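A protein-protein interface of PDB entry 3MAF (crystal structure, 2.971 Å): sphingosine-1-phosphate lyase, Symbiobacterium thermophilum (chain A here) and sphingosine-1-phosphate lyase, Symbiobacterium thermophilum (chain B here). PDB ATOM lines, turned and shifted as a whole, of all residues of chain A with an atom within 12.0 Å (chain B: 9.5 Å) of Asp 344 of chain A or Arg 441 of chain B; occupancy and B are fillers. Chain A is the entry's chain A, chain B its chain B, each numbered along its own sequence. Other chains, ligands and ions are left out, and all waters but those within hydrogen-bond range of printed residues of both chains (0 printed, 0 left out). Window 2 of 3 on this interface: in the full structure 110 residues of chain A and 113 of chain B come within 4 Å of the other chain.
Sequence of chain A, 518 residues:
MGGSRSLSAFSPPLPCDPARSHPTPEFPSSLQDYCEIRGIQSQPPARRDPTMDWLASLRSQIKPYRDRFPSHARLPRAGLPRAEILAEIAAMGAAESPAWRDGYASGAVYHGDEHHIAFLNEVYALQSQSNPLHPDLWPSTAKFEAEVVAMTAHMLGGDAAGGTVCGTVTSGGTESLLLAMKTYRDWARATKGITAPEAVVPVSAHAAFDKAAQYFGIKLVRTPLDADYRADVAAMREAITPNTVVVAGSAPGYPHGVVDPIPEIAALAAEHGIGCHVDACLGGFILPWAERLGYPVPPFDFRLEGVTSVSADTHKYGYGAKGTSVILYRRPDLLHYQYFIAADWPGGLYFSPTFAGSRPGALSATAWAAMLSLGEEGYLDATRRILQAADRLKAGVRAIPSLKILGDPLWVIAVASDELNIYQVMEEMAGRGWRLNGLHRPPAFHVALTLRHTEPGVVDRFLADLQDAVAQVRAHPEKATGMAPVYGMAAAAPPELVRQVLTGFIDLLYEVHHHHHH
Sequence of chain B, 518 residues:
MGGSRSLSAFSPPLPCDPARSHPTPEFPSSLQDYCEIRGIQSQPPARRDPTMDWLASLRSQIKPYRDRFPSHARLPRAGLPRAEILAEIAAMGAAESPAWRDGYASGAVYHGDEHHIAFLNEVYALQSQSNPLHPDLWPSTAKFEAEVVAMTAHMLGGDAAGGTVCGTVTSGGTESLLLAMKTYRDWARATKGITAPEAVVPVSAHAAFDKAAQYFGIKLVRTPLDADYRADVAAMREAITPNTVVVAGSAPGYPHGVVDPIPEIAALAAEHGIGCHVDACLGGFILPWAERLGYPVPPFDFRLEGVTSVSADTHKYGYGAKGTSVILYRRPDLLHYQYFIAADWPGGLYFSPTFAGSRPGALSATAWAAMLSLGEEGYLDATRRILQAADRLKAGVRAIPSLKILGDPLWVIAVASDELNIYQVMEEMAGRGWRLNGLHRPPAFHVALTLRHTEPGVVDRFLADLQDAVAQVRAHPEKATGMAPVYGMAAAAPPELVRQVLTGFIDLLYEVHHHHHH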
ATOM      1  N   PHE A 340      38.865  11.212  12.277  1.00  0.00           N
ATOM      2  CA  PHE A 340      37.806  10.469  12.948  1.00  0.00           C
ATOM      3  C   PHE A 340      37.041   9.608  11.955  1.00  0.00           C
ATOM      4  O   PHE A 340      36.612  10.087  10.900  1.00  0.00           O
ATOM      5  CB  PHE A 340      36.817  11.397  13.643  1.00  0.00           C
ATOM      6  CG  PHE A 340      35.493  10.743  13.926  1.00  0.00           C
ATOM      7  CD1 PHE A 340      35.312   9.993  15.078  1.00  0.00           C
ATOM      8  CD2 PHE A 340      34.436  10.847  13.020  1.00  0.00           C
ATOM      9  CE1 PHE A 340      34.099   9.369  15.337  1.00  0.00           C
ATOM     10  CE2 PHE A 340      33.214  10.230  13.270  1.00  0.00           C
ATOM     11  CZ  PHE A 340      33.047   9.488  14.433  1.00  0.00           C
ATOM     12  N   ILE A 341      36.845   8.345  12.308  1.00  0.00           N
ATOM     13  CA  ILE A 341      36.114   7.422  11.446  1.00  0.00           C
ATOM     14  C   ILE A 341      35.104   6.602  12.241  1.00  0.00           C
ATOM     15  O   ILE A 341      35.397   6.129  13.348  1.00  0.00           O
ATOM     16  CB  ILE A 341      37.070   6.461  10.717  1.00  0.00           C
ATOM     17  CG1 ILE A 341      38.036   7.251   9.846  1.00  0.00           C
ATOM     18  CG2 ILE A 341      36.299   5.490   9.858  1.00  0.00           C
ATOM     19  CD1 ILE A 341      39.082   6.392   9.193  1.00  0.00           C
ATOM     20  N   ALA A 342      33.913   6.444  11.671  1.00  0.00           N
ATOM     21  CA  ALA A 342      32.868   5.633  12.282  1.00  0.00           C
ATOM     22  C   ALA A 342      32.385   4.596  11.285  1.00  0.00           C
ATOM     23  O   ALA A 342      31.905   4.933  10.196  1.00  0.00           O
ATOM     24  CB  ALA A 342      31.713   6.501  12.739  1.00  0.00           C
ATOM     25  N   ALA A 343      32.508   3.331  11.668  1.00  0.00           N
ATOM     26  CA  ALA A 343      32.174   2.226  10.778  1.00  0.00           C
ATOM     27  C   ALA A 343      30.680   1.915  10.729  1.00  0.00           C
ATOM     28  O   ALA A 343      30.018   2.202   9.736  1.00  0.00           O
ATOM     29  CB  ALA A 343      32.961   0.987  11.161  1.00  0.00           C
ATOM     30  N   ASP A 344      30.148   1.338  11.805  1.00  0.00           N
ATOM     31  CA  ASP A 344      28.792   0.785  11.780  1.00  0.00           C
ATOM     32  C   ASP A 344      27.675   1.759  12.183  1.00  0.00           C
ATOM     33  O   ASP A 344      26.750   1.418  12.928  1.00  0.00           O
ATOM     34  CB  ASP A 344      28.724  -0.497  12.607  1.00  0.00           C
ATOM     35  CG  ASP A 344      29.325  -0.328  13.972  1.00  0.00           C
ATOM     36  OD1 ASP A 344      29.392   0.827  14.447  1.00  0.00           O
ATOM     37  OD2 ASP A 344      29.726  -1.350  14.567  1.00  0.00           O
ATOM     38  N   TRP A 345      27.763   2.972  11.663  1.00  0.00           N
ATOM     39  CA  TRP A 345      26.656   3.899  11.734  1.00  0.00           C
ATOM     40  C   TRP A 345      25.702   3.579  10.583  1.00  0.00           C
ATOM     41  O   TRP A 345      26.119   3.470   9.429  1.00  0.00           O
ATOM     42  CB  TRP A 345      27.171   5.328  11.617  1.00  0.00           C
ATOM     43  CG  TRP A 345      26.098   6.349  11.692  1.00  0.00           C
ATOM     44  CD1 TRP A 345      25.067   6.385  12.579  1.00  0.00           C
ATOM     45  CD2 TRP A 345      25.952   7.503  10.859  1.00  0.00           C
ATOM     46  NE1 TRP A 345      24.279   7.487  12.349  1.00  0.00           N
ATOM     47  CE2 TRP A 345      24.803   8.193  11.300  1.00  0.00           C
ATOM     48  CE3 TRP A 345      26.681   8.022   9.784  1.00  0.00           C
ATOM     49  CZ2 TRP A 345      24.365   9.375  10.706  1.00  0.00           C
ATOM     50  CZ3 TRP A 345      26.246   9.196   9.194  1.00  0.00           C
ATOM     51  CH2 TRP A 345      25.096   9.860   9.656  1.00  0.00           C
ATOM     52  N   PRO A 346      24.415   3.406  10.891  1.00  0.00           N
ATOM     53  CA  PRO A 346      23.416   3.126   9.857  1.00  0.00           C
ATOM     54  C   PRO A 346      23.407   4.186   8.758  1.00  0.00           C
ATOM     55  O   PRO A 346      22.835   3.966   7.690  1.00  0.00           O
ATOM     56  CB  PRO A 346      22.102   3.164  10.632  1.00  0.00           C
ATOM     57  CG  PRO A 346      22.477   2.798  12.012  1.00  0.00           C
ATOM     58  CD  PRO A 346      23.835   3.376  12.244  1.00  0.00           C
ATOM     59  N   GLY A 347      24.034   5.327   9.014  1.00  0.00           N
ATOM     60  CA  GLY A 347      24.068   6.400   8.037  1.00  0.00           C
ATOM     61  C   GLY A 347      25.162   6.208   7.007  1.00  0.00           C
ATOM     62  O   GLY A 347      25.395   7.068   6.158  1.00  0.00           O
ATOM     63  N   GLY A 348      25.837   5.069   7.084  1.00  0.00           N
ATOM     64  CA  GLY A 348      26.890   4.757   6.144  1.00  0.00           C
ATOM     65  C   GLY A 348      28.248   4.947   6.769  1.00  0.00           C
ATOM     66  O   GLY A 348      28.358   5.289   7.949  1.00  0.00           O
ATOM     67  N   LEU A 349      29.290   4.704   5.983  1.00  0.00           N
ATOM     68  CA  LEU A 349      30.652   4.935   6.442  1.00  0.00           C
ATOM     69  C   LEU A 349      30.821   6.425   6.684  1.00  0.00           C
ATOM     70  O   LEU A 349      30.354   7.257   5.889  1.00  0.00           O
ATOM     71  CB  LEU A 349      31.659   4.447   5.409  1.00  0.00           C
ATOM     72  CG  LEU A 349      31.484   2.979   5.024  1.00  0.00           C
ATOM     73  CD1 LEU A 349      32.084   2.684   3.654  1.00  0.00           C
ATOM     74  CD2 LEU A 349      32.091   2.088   6.093  1.00  0.00           C
ATOM     75  N   TYR A 350      31.466   6.765   7.793  1.00  0.00           N
ATOM     76  CA  TYR A 350      31.652   8.162   8.142  1.00  0.00           C
ATOM     77  C   TYR A 350      33.107   8.482   8.470  1.00  0.00           C
ATOM     78  O   TYR A 350      33.699   7.906   9.392  1.00  0.00           O
ATOM     79  CB  TYR A 350      30.744   8.567   9.310  1.00  0.00           C
ATOM     80  CG  TYR A 350      30.609  10.069   9.461  1.00  0.00           C
ATOM     81  CD1 TYR A 350      29.755  10.803   8.629  1.00  0.00           C
ATOM     82  CD2 TYR A 350      31.344  10.757  10.416  1.00  0.00           C
ATOM     83  CE1 TYR A 350      29.639  12.180   8.751  1.00  0.00           C
ATOM     84  CE2 TYR A 350      31.235  12.136  10.551  1.00  0.00           C
ATOM     85  CZ  TYR A 350      30.384  12.844   9.716  1.00  0.00           C
ATOM     86  OH  TYR A 350      30.281  14.216   9.854  1.00  0.00           O
ATOM     87  N   PHE A 351      33.680   9.404   7.703  1.00  0.00           N
ATOM     88  CA  PHE A 351      34.986   9.933   8.038  1.00  0.00           C
ATOM     89  C   PHE A 351      34.947  11.444   8.057  1.00  0.00           C
ATOM     90  O   PHE A 351      34.200  12.066   7.303  1.00  0.00           O
ATOM     91  CB  PHE A 351      36.068   9.435   7.069  1.00  0.00           C
ATOM     92  CG  PHE A 351      35.926   9.960   5.660  1.00  0.00           C
ATOM     93  CD1 PHE A 351      35.327   9.186   4.669  1.00  0.00           C
ATOM     94  CD2 PHE A 351      36.408  11.219   5.316  1.00  0.00           C
ATOM     95  CE1 PHE A 351      35.200   9.660   3.363  1.00  0.00           C
ATOM     96  CE2 PHE A 351      36.285  11.703   4.010  1.00  0.00           C
ATOM     97  CZ  PHE A 351      35.680  10.920   3.033  1.00  0.00           C
ATOM     98  N   PRO B 202      19.973   6.972  20.442  1.00  0.00           N
ATOM     99  CA  PRO B 202      19.566   5.896  19.536  1.00  0.00           C
ATOM    100  C   PRO B 202      20.702   5.589  18.575  1.00  0.00           C
ATOM    101  O   PRO B 202      21.482   6.472  18.207  1.00  0.00           O
ATOM    102  CB  PRO B 202      18.390   6.501  18.770  1.00  0.00           C
ATOM    103  CG  PRO B 202      17.892   7.587  19.646  1.00  0.00           C
ATOM    104  CD  PRO B 202      19.080   8.136  20.360  1.00  0.00           C
ATOM    105  N   VAL B 203      20.802   4.331  18.179  1.00  0.00           N
ATOM    106  CA  VAL B 203      21.825   3.915  17.240  1.00  0.00           C
ATOM    107  C   VAL B 203      21.769   4.781  15.966  1.00  0.00           C
ATOM    108  O   VAL B 203      22.782   4.980  15.289  1.00  0.00           O
ATOM    109  CB  VAL B 203      21.651   2.423  16.906  1.00  0.00           C
ATOM    110  CG1 VAL B 203      20.399   2.213  16.064  1.00  0.00           C
ATOM    111  CG2 VAL B 203      22.874   1.884  16.199  1.00  0.00           C
ATOM    112  N   SER B 204      20.587   5.310  15.660  1.00  0.00           N
ATOM    113  CA  SER B 204      20.386   6.133  14.467  1.00  0.00           C
ATOM    114  C   SER B 204      21.005   7.530  14.602  1.00  0.00           C
ATOM    115  O   SER B 204      21.239   8.213  13.599  1.00  0.00           O
ATOM    116  CB  SER B 204      18.894   6.257  14.159  1.00  0.00           C
ATOM    117  OG  SER B 204      18.201   6.850  15.254  1.00  0.00           O
ATOM    118  N   ALA B 205      21.263   7.937  15.845  1.00  0.00           N
ATOM    119  CA  ALA B 205      21.771   9.268  16.154  1.00  0.00           C
ATOM    120  C   ALA B 205      23.041   9.586  15.381  1.00  0.00           C
ATOM    121  O   ALA B 205      23.917   8.741  15.245  1.00  0.00           O
ATOM    122  CB  ALA B 205      22.018   9.395  17.632  1.00  0.00           C
ATOM    123  N   ALA B 207      26.454  10.405  13.561  1.00  0.00           N
ATOM    124  CA  ALA B 207      27.798   9.932  13.867  1.00  0.00           C
ATOM    125  C   ALA B 207      28.649  10.964  14.611  1.00  0.00           C
ATOM    126  O   ALA B 207      29.579  10.604  15.334  1.00  0.00           O
ATOM    127  CB  ALA B 207      28.486   9.500  12.599  1.00  0.00           C
ATOM    128  N   ASP B 210      29.564  10.295  18.120  1.00  0.00           N
ATOM    129  CA  ASP B 210      30.687   9.449  18.459  1.00  0.00           C
ATOM    130  C   ASP B 210      31.964  10.279  18.546  1.00  0.00           C
ATOM    131  O   ASP B 210      32.833  10.000  19.386  1.00  0.00           O
ATOM    132  CB  ASP B 210      30.821   8.320  17.446  1.00  0.00           C
ATOM    133  CG  ASP B 210      29.702   7.293  17.567  1.00  0.00           C
ATOM    134  OD1 ASP B 210      28.847   7.239  16.658  1.00  0.00           O
ATOM    135  OD2 ASP B 210      29.674   6.544  18.569  1.00  0.00           O
ATOM    136  N   LEU B 220      29.631   6.769  25.160  1.00  0.00           N
ATOM    137  CA  LEU B 220      28.413   6.883  24.363  1.00  0.00           C
ATOM    138  C   LEU B 220      27.725   5.532  24.273  1.00  0.00           C
ATOM    139  O   LEU B 220      28.329   4.536  23.850  1.00  0.00           O
ATOM    140  CB  LEU B 220      28.716   7.411  22.962  1.00  0.00           C
ATOM    141  CG  LEU B 220      27.470   7.557  22.094  1.00  0.00           C
ATOM    142  CD1 LEU B 220      26.629   8.701  22.623  1.00  0.00           C
ATOM    143  CD2 LEU B 220      27.841   7.789  20.632  1.00  0.00           C
ATOM    144  N   ARG B 222      24.672   3.609  22.561  1.00  0.00           N
ATOM    145  CA  ARG B 222      23.670   3.650  21.505  1.00  0.00           C
ATOM    146  C   ARG B 222      22.617   2.564  21.722  1.00  0.00           C
ATOM    147  O   ARG B 222      22.934   1.383  21.819  1.00  0.00           O
ATOM    148  CB  ARG B 222      24.324   3.512  20.127  1.00  0.00           C
ATOM    149  CG  ARG B 222      25.162   4.706  19.726  1.00  0.00           C
ATOM    150  CD  ARG B 222      25.661   4.583  18.294  1.00  0.00           C
ATOM    151  NE  ARG B 222      26.260   5.825  17.816  1.00  0.00           N
ATOM    152  CZ  ARG B 222      25.574   6.816  17.254  1.00  0.00           C
ATOM    153  NH1 ARG B 222      24.262   6.717  17.093  1.00  0.00           N
ATOM    154  NH2 ARG B 222      26.200   7.907  16.848  1.00  0.00           N
ATOM    155  N   LEU B 225      16.655   0.531  17.825  1.00  0.00           N
ATOM    156  CA  LEU B 225      15.465   1.128  17.241  1.00  0.00           C
ATOM    157  C   LEU B 225      14.323   0.144  17.326  1.00  0.00           C
ATOM    158  O   LEU B 225      14.533  -1.035  17.609  1.00  0.00           O
ATOM    159  CB  LEU B 225      15.689   1.468  15.772  1.00  0.00           C
ATOM    160  CG  LEU B 225      16.830   2.413  15.429  1.00  0.00           C
ATOM    161  CD1 LEU B 225      16.709   2.818  13.969  1.00  0.00           C
ATOM    162  CD2 LEU B 225      16.809   3.630  16.352  1.00  0.00           C
ATOM    163  N   TYR B 229      11.763   1.966  13.034  1.00  0.00           N
ATOM    164  CA  TYR B 229      13.043   2.661  12.989  1.00  0.00           C
ATOM    165  C   TYR B 229      13.040   3.948  13.798  1.00  0.00           C
ATOM    166  O   TYR B 229      13.728   4.915  13.460  1.00  0.00           O
ATOM    167  CB  TYR B 229      13.457   2.923  11.539  1.00  0.00           C
ATOM    168  CG  TYR B 229      13.758   1.650  10.785  1.00  0.00           C
ATOM    169  CD1 TYR B 229      15.063   1.200  10.641  1.00  0.00           C
ATOM    170  CD2 TYR B 229      12.737   0.886  10.234  1.00  0.00           C
ATOM    171  CE1 TYR B 229      15.341   0.030   9.959  1.00  0.00           C
ATOM    172  CE2 TYR B 229      13.005  -0.281   9.553  1.00  0.00           C
ATOM    173  CZ  TYR B 229      14.306  -0.707   9.422  1.00  0.00           C
ATOM    174  OH  TYR B 229      14.578  -1.873   8.748  1.00  0.00           O
ATOM    175  N   PRO B 255      19.947   8.953   8.838  1.00  0.00           N
ATOM    176  CA  PRO B 255      19.886   7.656   8.156  1.00  0.00           C
ATOM    177  C   PRO B 255      18.545   7.407   7.480  1.00  0.00           C
ATOM    178  O   PRO B 255      18.497   7.232   6.259  1.00  0.00           O
ATOM    179  CB  PRO B 255      20.095   6.650   9.287  1.00  0.00           C
ATOM    180  CG  PRO B 255      20.840   7.389  10.318  1.00  0.00           C
ATOM    181  CD  PRO B 255      20.368   8.813  10.243  1.00  0.00           C
ATOM    182  N   HIS B 256      17.466   7.410   8.258  1.00  0.00           N
ATOM    183  CA  HIS B 256      16.167   7.001   7.728  1.00  0.00           C
ATOM    184  C   HIS B 256      15.124   8.106   7.676  1.00  0.00           C
ATOM    185  O   HIS B 256      14.021   7.902   7.166  1.00  0.00           O
ATOM    186  CB  HIS B 256      15.652   5.798   8.501  1.00  0.00           C
ATOM    187  CG  HIS B 256      16.663   4.705   8.624  1.00  0.00           C
ATOM    188  ND1 HIS B 256      17.002   4.136   9.832  1.00  0.00           N
ATOM    189  CD2 HIS B 256      17.440   4.104   7.692  1.00  0.00           C
ATOM    190  CE1 HIS B 256      17.926   3.212   9.637  1.00  0.00           C
ATOM    191  NE2 HIS B 256      18.212   3.175   8.347  1.00  0.00           N
ATOM    192  N   LEU B 406      12.055   2.342   4.539  1.00  0.00           N
ATOM    193  CA  LEU B 406      12.300   2.165   5.960  1.00  0.00           C
ATOM    194  C   LEU B 406      11.601   3.234   6.785  1.00  0.00           C
ATOM    195  O   LEU B 406      11.783   4.424   6.553  1.00  0.00           O
ATOM    196  CB  LEU B 406      13.796   2.231   6.229  1.00  0.00           C
ATOM    197  CG  LEU B 406      14.619   1.277   5.372  1.00  0.00           C
ATOM    198  CD1 LEU B 406      16.090   1.402   5.717  1.00  0.00           C
ATOM    199  CD2 LEU B 406      14.131  -0.151   5.566  1.00  0.00           C
ATOM    200  N   ALA B 416      15.059   0.370   0.713  1.00  0.00           N
ATOM    201  CA  ALA B 416      15.819  -0.876   0.671  1.00  0.00           C
ATOM    202  C   ALA B 416      15.054  -2.006  -0.031  1.00  0.00           C
ATOM    203  O   ALA B 416      13.884  -1.864  -0.386  1.00  0.00           O
ATOM    204  CB  ALA B 416      16.204  -1.298   2.074  1.00  0.00           C
ATOM    205  N   ILE B 422      20.066  -3.914  -3.074  1.00  0.00           N
ATOM    206  CA  ILE B 422      19.797  -2.483  -3.130  1.00  0.00           C
ATOM    207  C   ILE B 422      21.008  -1.663  -3.582  1.00  0.00           C
ATOM    208  O   ILE B 422      20.850  -0.622  -4.221  1.00  0.00           O
ATOM    209  CB  ILE B 422      19.317  -1.952  -1.766  1.00  0.00           C
ATOM    210  CG1 ILE B 422      18.619  -0.601  -1.934  1.00  0.00           C
ATOM    211  CG2 ILE B 422      20.488  -1.846  -0.804  1.00  0.00           C
ATOM    212  CD1 ILE B 422      17.365  -0.676  -2.747  1.00  0.00           C
ATOM    213  N   TYR B 423      22.211  -2.118  -3.246  1.00  0.00           N
ATOM    214  CA  TYR B 423      23.414  -1.384  -3.629  1.00  0.00           C
ATOM    215  C   TYR B 423      23.563  -1.360  -5.141  1.00  0.00           C
ATOM    216  O   TYR B 423      24.060  -0.388  -5.713  1.00  0.00           O
ATOM    217  CB  TYR B 423      24.657  -1.981  -2.975  1.00  0.00           C
ATOM    218  CG  TYR B 423      24.690  -1.806  -1.482  1.00  0.00           C
ATOM    219  CD1 TYR B 423      24.470  -0.564  -0.910  1.00  0.00           C
ATOM    220  CD2 TYR B 423      24.947  -2.874  -0.644  1.00  0.00           C
ATOM    221  CE1 TYR B 423      24.493  -0.391   0.453  1.00  0.00           C
ATOM    222  CE2 TYR B 423      24.978  -2.712   0.724  1.00  0.00           C
ATOM    223  CZ  TYR B 423      24.746  -1.467   1.270  1.00  0.00           C
ATOM    224  OH  TYR B 423      24.770  -1.299   2.641  1.00  0.00           O
ATOM    225  N   GLY B 438      24.477   5.946   0.090  1.00  0.00           N
ATOM    226  CA  GLY B 438      24.352   4.556   0.480  1.00  0.00           C
ATOM    227  C   GLY B 438      24.442   4.377   1.984  1.00  0.00           C
ATOM    228  O   GLY B 438      25.372   4.846   2.634  1.00  0.00           O
ATOM    229  N   LEU B 439      23.458   3.693   2.547  1.00  0.00           N
ATOM    230  CA  LEU B 439      23.426   3.443   3.975  1.00  0.00           C
ATOM    231  C   LEU B 439      23.752   1.985   4.203  1.00  0.00           C
ATOM    232  O   LEU B 439      23.749   1.199   3.260  1.00  0.00           O
ATOM    233  CB  LEU B 439      22.030   3.734   4.520  1.00  0.00           C
ATOM    234  CG  LEU B 439      21.372   4.993   3.959  1.00  0.00           C
ATOM    235  CD1 LEU B 439      19.868   4.903   4.065  1.00  0.00           C
ATOM    236  CD2 LEU B 439      21.901   6.228   4.664  1.00  0.00           C
ATOM    237  N   HIS B 440      24.032   1.617   5.448  1.00  0.00           N
ATOM    238  CA  HIS B 440      24.157   0.208   5.776  1.00  0.00           C
ATOM    239  C   HIS B 440      23.591  -0.064   7.158  1.00  0.00           C
ATOM    240  O   HIS B 440      23.240   0.871   7.879  1.00  0.00           O
ATOM    241  CB  HIS B 440      25.602  -0.250   5.682  1.00  0.00           C
ATOM    242  CG  HIS B 440      26.535   0.512   6.566  1.00  0.00           C
ATOM    243  ND1 HIS B 440      27.657   1.153   6.085  1.00  0.00           N
ATOM    244  CD2 HIS B 440      26.514   0.737   7.900  1.00  0.00           C
ATOM    245  CE1 HIS B 440      28.291   1.735   7.087  1.00  0.00           C
ATOM    246  NE2 HIS B 440      27.617   1.498   8.200  1.00  0.00           N
ATOM    247  N   ARG B 441      23.491  -1.343   7.518  1.00  0.00           N
ATOM    248  CA  ARG B 441      22.902  -1.741   8.797  1.00  0.00           C
ATOM    249  C   ARG B 441      21.585  -1.024   9.052  1.00  0.00           C
ATOM    250  O   ARG B 441      21.474  -0.266  10.014  1.00  0.00           O
ATOM    251  CB  ARG B 441      23.857  -1.429   9.954  1.00  0.00           C
ATOM    252  CG  ARG B 441      25.185  -2.146   9.886  1.00  0.00           C
ATOM    253  CD  ARG B 441      25.903  -2.095  11.231  1.00  0.00           C
ATOM    254  NE  ARG B 441      27.219  -2.744  11.225  1.00  0.00           N
ATOM    255  CZ  ARG B 441      28.015  -2.871  10.160  1.00  0.00           C
ATOM    256  NH1 ARG B 441      27.656  -2.388   8.976  1.00  0.00           N
ATOM    257  NH2 ARG B 441      29.191  -3.480  10.280  1.00  0.00           N
ATOM    258  N   PRO B 442      20.573  -1.266   8.204  1.00  0.00           N
ATOM    259  CA  PRO B 442      20.554  -2.193   7.067  1.00  0.00           C
ATOM    260  C   PRO B 442      20.996  -1.540   5.763  1.00  0.00           C
ATOM    261  O   PRO B 442      21.162  -0.323   5.695  1.00  0.00           O
ATOM    262  CB  PRO B 442      19.063  -2.569   6.946  1.00  0.00           C
ATOM    263  CG  PRO B 442      18.341  -1.794   8.029  1.00  0.00           C
ATOM    264  CD  PRO B 442      19.250  -0.664   8.403  1.00  0.00           C
ATOM    265  N   PRO B 443      21.178  -2.350   4.722  1.00  0.00           N
ATOM    266  CA  PRO B 443      21.552  -1.838   3.406  1.00  0.00           C
ATOM    267  C   PRO B 443      20.393  -1.111   2.769  1.00  0.00           C
ATOM    268  O   PRO B 443      19.284  -1.631   2.743  1.00  0.00           O
ATOM    269  CB  PRO B 443      21.862  -3.109   2.613  1.00  0.00           C
ATOM    270  CG  PRO B 443      22.137  -4.142   3.646  1.00  0.00           C
ATOM    271  CD  PRO B 443      21.235  -3.814   4.778  1.00  0.00           C
ATOM    272  N   ALA B 444      20.664   0.080   2.252  1.00  0.00           N
ATOM    273  CA  ALA B 444      19.672   0.879   1.557  1.00  0.00           C
ATOM    274  C   ALA B 444      20.334   2.174   1.130  1.00  0.00           C
ATOM    275  O   ALA B 444      21.326   2.583   1.726  1.00  0.00           O
ATOM    276  CB  ALA B 444      18.497   1.173   2.470  1.00  0.00           C
ATOM    277  N   PHE B 445      19.799   2.818   0.101  1.00  0.00           N
ATOM    278  CA  PHE B 445      20.258   4.149  -0.260  1.00  0.00           C
ATOM    279  C   PHE B 445      19.199   5.138   0.194  1.00  0.00           C
ATOM    280  O   PHE B 445      18.065   4.750   0.446  1.00  0.00           O
ATOM    281  CB  PHE B 445      20.473   4.259  -1.767  1.00  0.00           C
ATOM    282  CG  PHE B 445      19.204   4.146  -2.570  1.00  0.00           C
ATOM    283  CD1 PHE B 445      18.328   5.220  -2.667  1.00  0.00           C
ATOM    284  CD2 PHE B 445      18.886   2.968  -3.226  1.00  0.00           C
ATOM    285  CE1 PHE B 445      17.164   5.120  -3.403  1.00  0.00           C
ATOM    286  CE2 PHE B 445      17.720   2.864  -3.963  1.00  0.00           C
ATOM    287  CZ  PHE B 445      16.857   3.940  -4.049  1.00  0.00           C
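O of Trp 345 of chain A lies within hydrogen-bond range of NE2 of His 440 of chain B.
The backbone NH (N) of His 440 of chain B lies within hydrogen-bond range of the backbone carbonyl oxygen (O) of Pro 346 of chain A (3.5 Å).
The backbone carbonyl oxygen (O) of Ala 343 of chain A sits at hydrogen-bond distance from a ring nitrogen (NE2) of His 440 of chain B, at 2.9 Å.
NE1 of Trp 345 of chain A lies within hydrogen-bond range of O of Ser 204 of chain B, at 3.4 Å.
The backbone carbonyl oxygen of Ala 205 of chain B lies within hydrogen-bond range of the indole nitrogen of Trp 345 of chain A (3.2 Å).
NH1 of Arg 222 of chain B lies within hydrogen-bond range of O of Val 203 of chain B (2.9 Å).
The backbone carbonyl oxygen of Ala 205 of chain B is in hydrogen-bond range of the guanidinium group of Arg 222 of chain B, at 2.8 Å.
Among the printed residues, pairs that only touch across the chains: Asp 344 of chain A with Arg 441 of chain B (3.0 Å), Gly 348 of chain A with His 440 of chain B (3.2 Å), Pro 346 of chain A with Leu 439 of chain B (3.3 Å), Leu 349 of chain A with His 440 of chain B (3.3 Å), Pro 346 of chain A with Arg 441 of chain B (3.5 Å), Trp 345 of chain A with Ala 207 of chain B (3.6 Å), Pro 346 of chain A with Val 203 of chain B (3.6 Å), Phe 340 of chain A with Ala 207 of chain B (3.8 Å), Tyr 350 of chain A with Ala 207 of chain B (3.8 Å), Trp 345 of chain A with Val 203 of chain B (3.8 Å), Gly 348 of chain A with Gly 438 of chain B (3.8 Å), Asp 344 of chain A with His 440 of chain B (3.8 Å), Gly 347 of chain A with Leu 439 of chain B (3.9 Å), Phe 340 of chain A with Asp 210 of chain B (3.9 Å) and Trp 345 of chain A with Pro 255 of chain B (3.995 Å).
Of chain B, only His 440 (3.8 Å) and Arg 441 (3.0 Å) come within 4 Å of Asp 344 of chain A.
His 440 of chain B touches six residues of chain A.
No residue of chain A comes within 4 Å of Pro 442 of chain B.
No residue of chain A comes within 4 Å of Ala 444 of chain B.
Of the printed residues of chain B, Leu 349 of chain A touches His 440.
Of the printed residues of chain A, Ser 204 of chain B touches Trp 345.
Leu 406 of chain B touches none of the printed residues of chain A.
The nearest residue of chain B that does not touch Asp 344 of chain A is Val 203 of chain B (5.1 Å).
Hydrophobic or aromatic side chains of chain B within 4 Å of the printed part of chain A: Ala 207, Pro 255, Leu 439 and His 440.
Along chain B the printed residues that touch a printed residue of chain A span positions 203 to 441.
Among the printed residues, no Asp or Glu carboxylate lies within 4 Å of a Lys or Arg side-chain nitrogen of the other chain.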
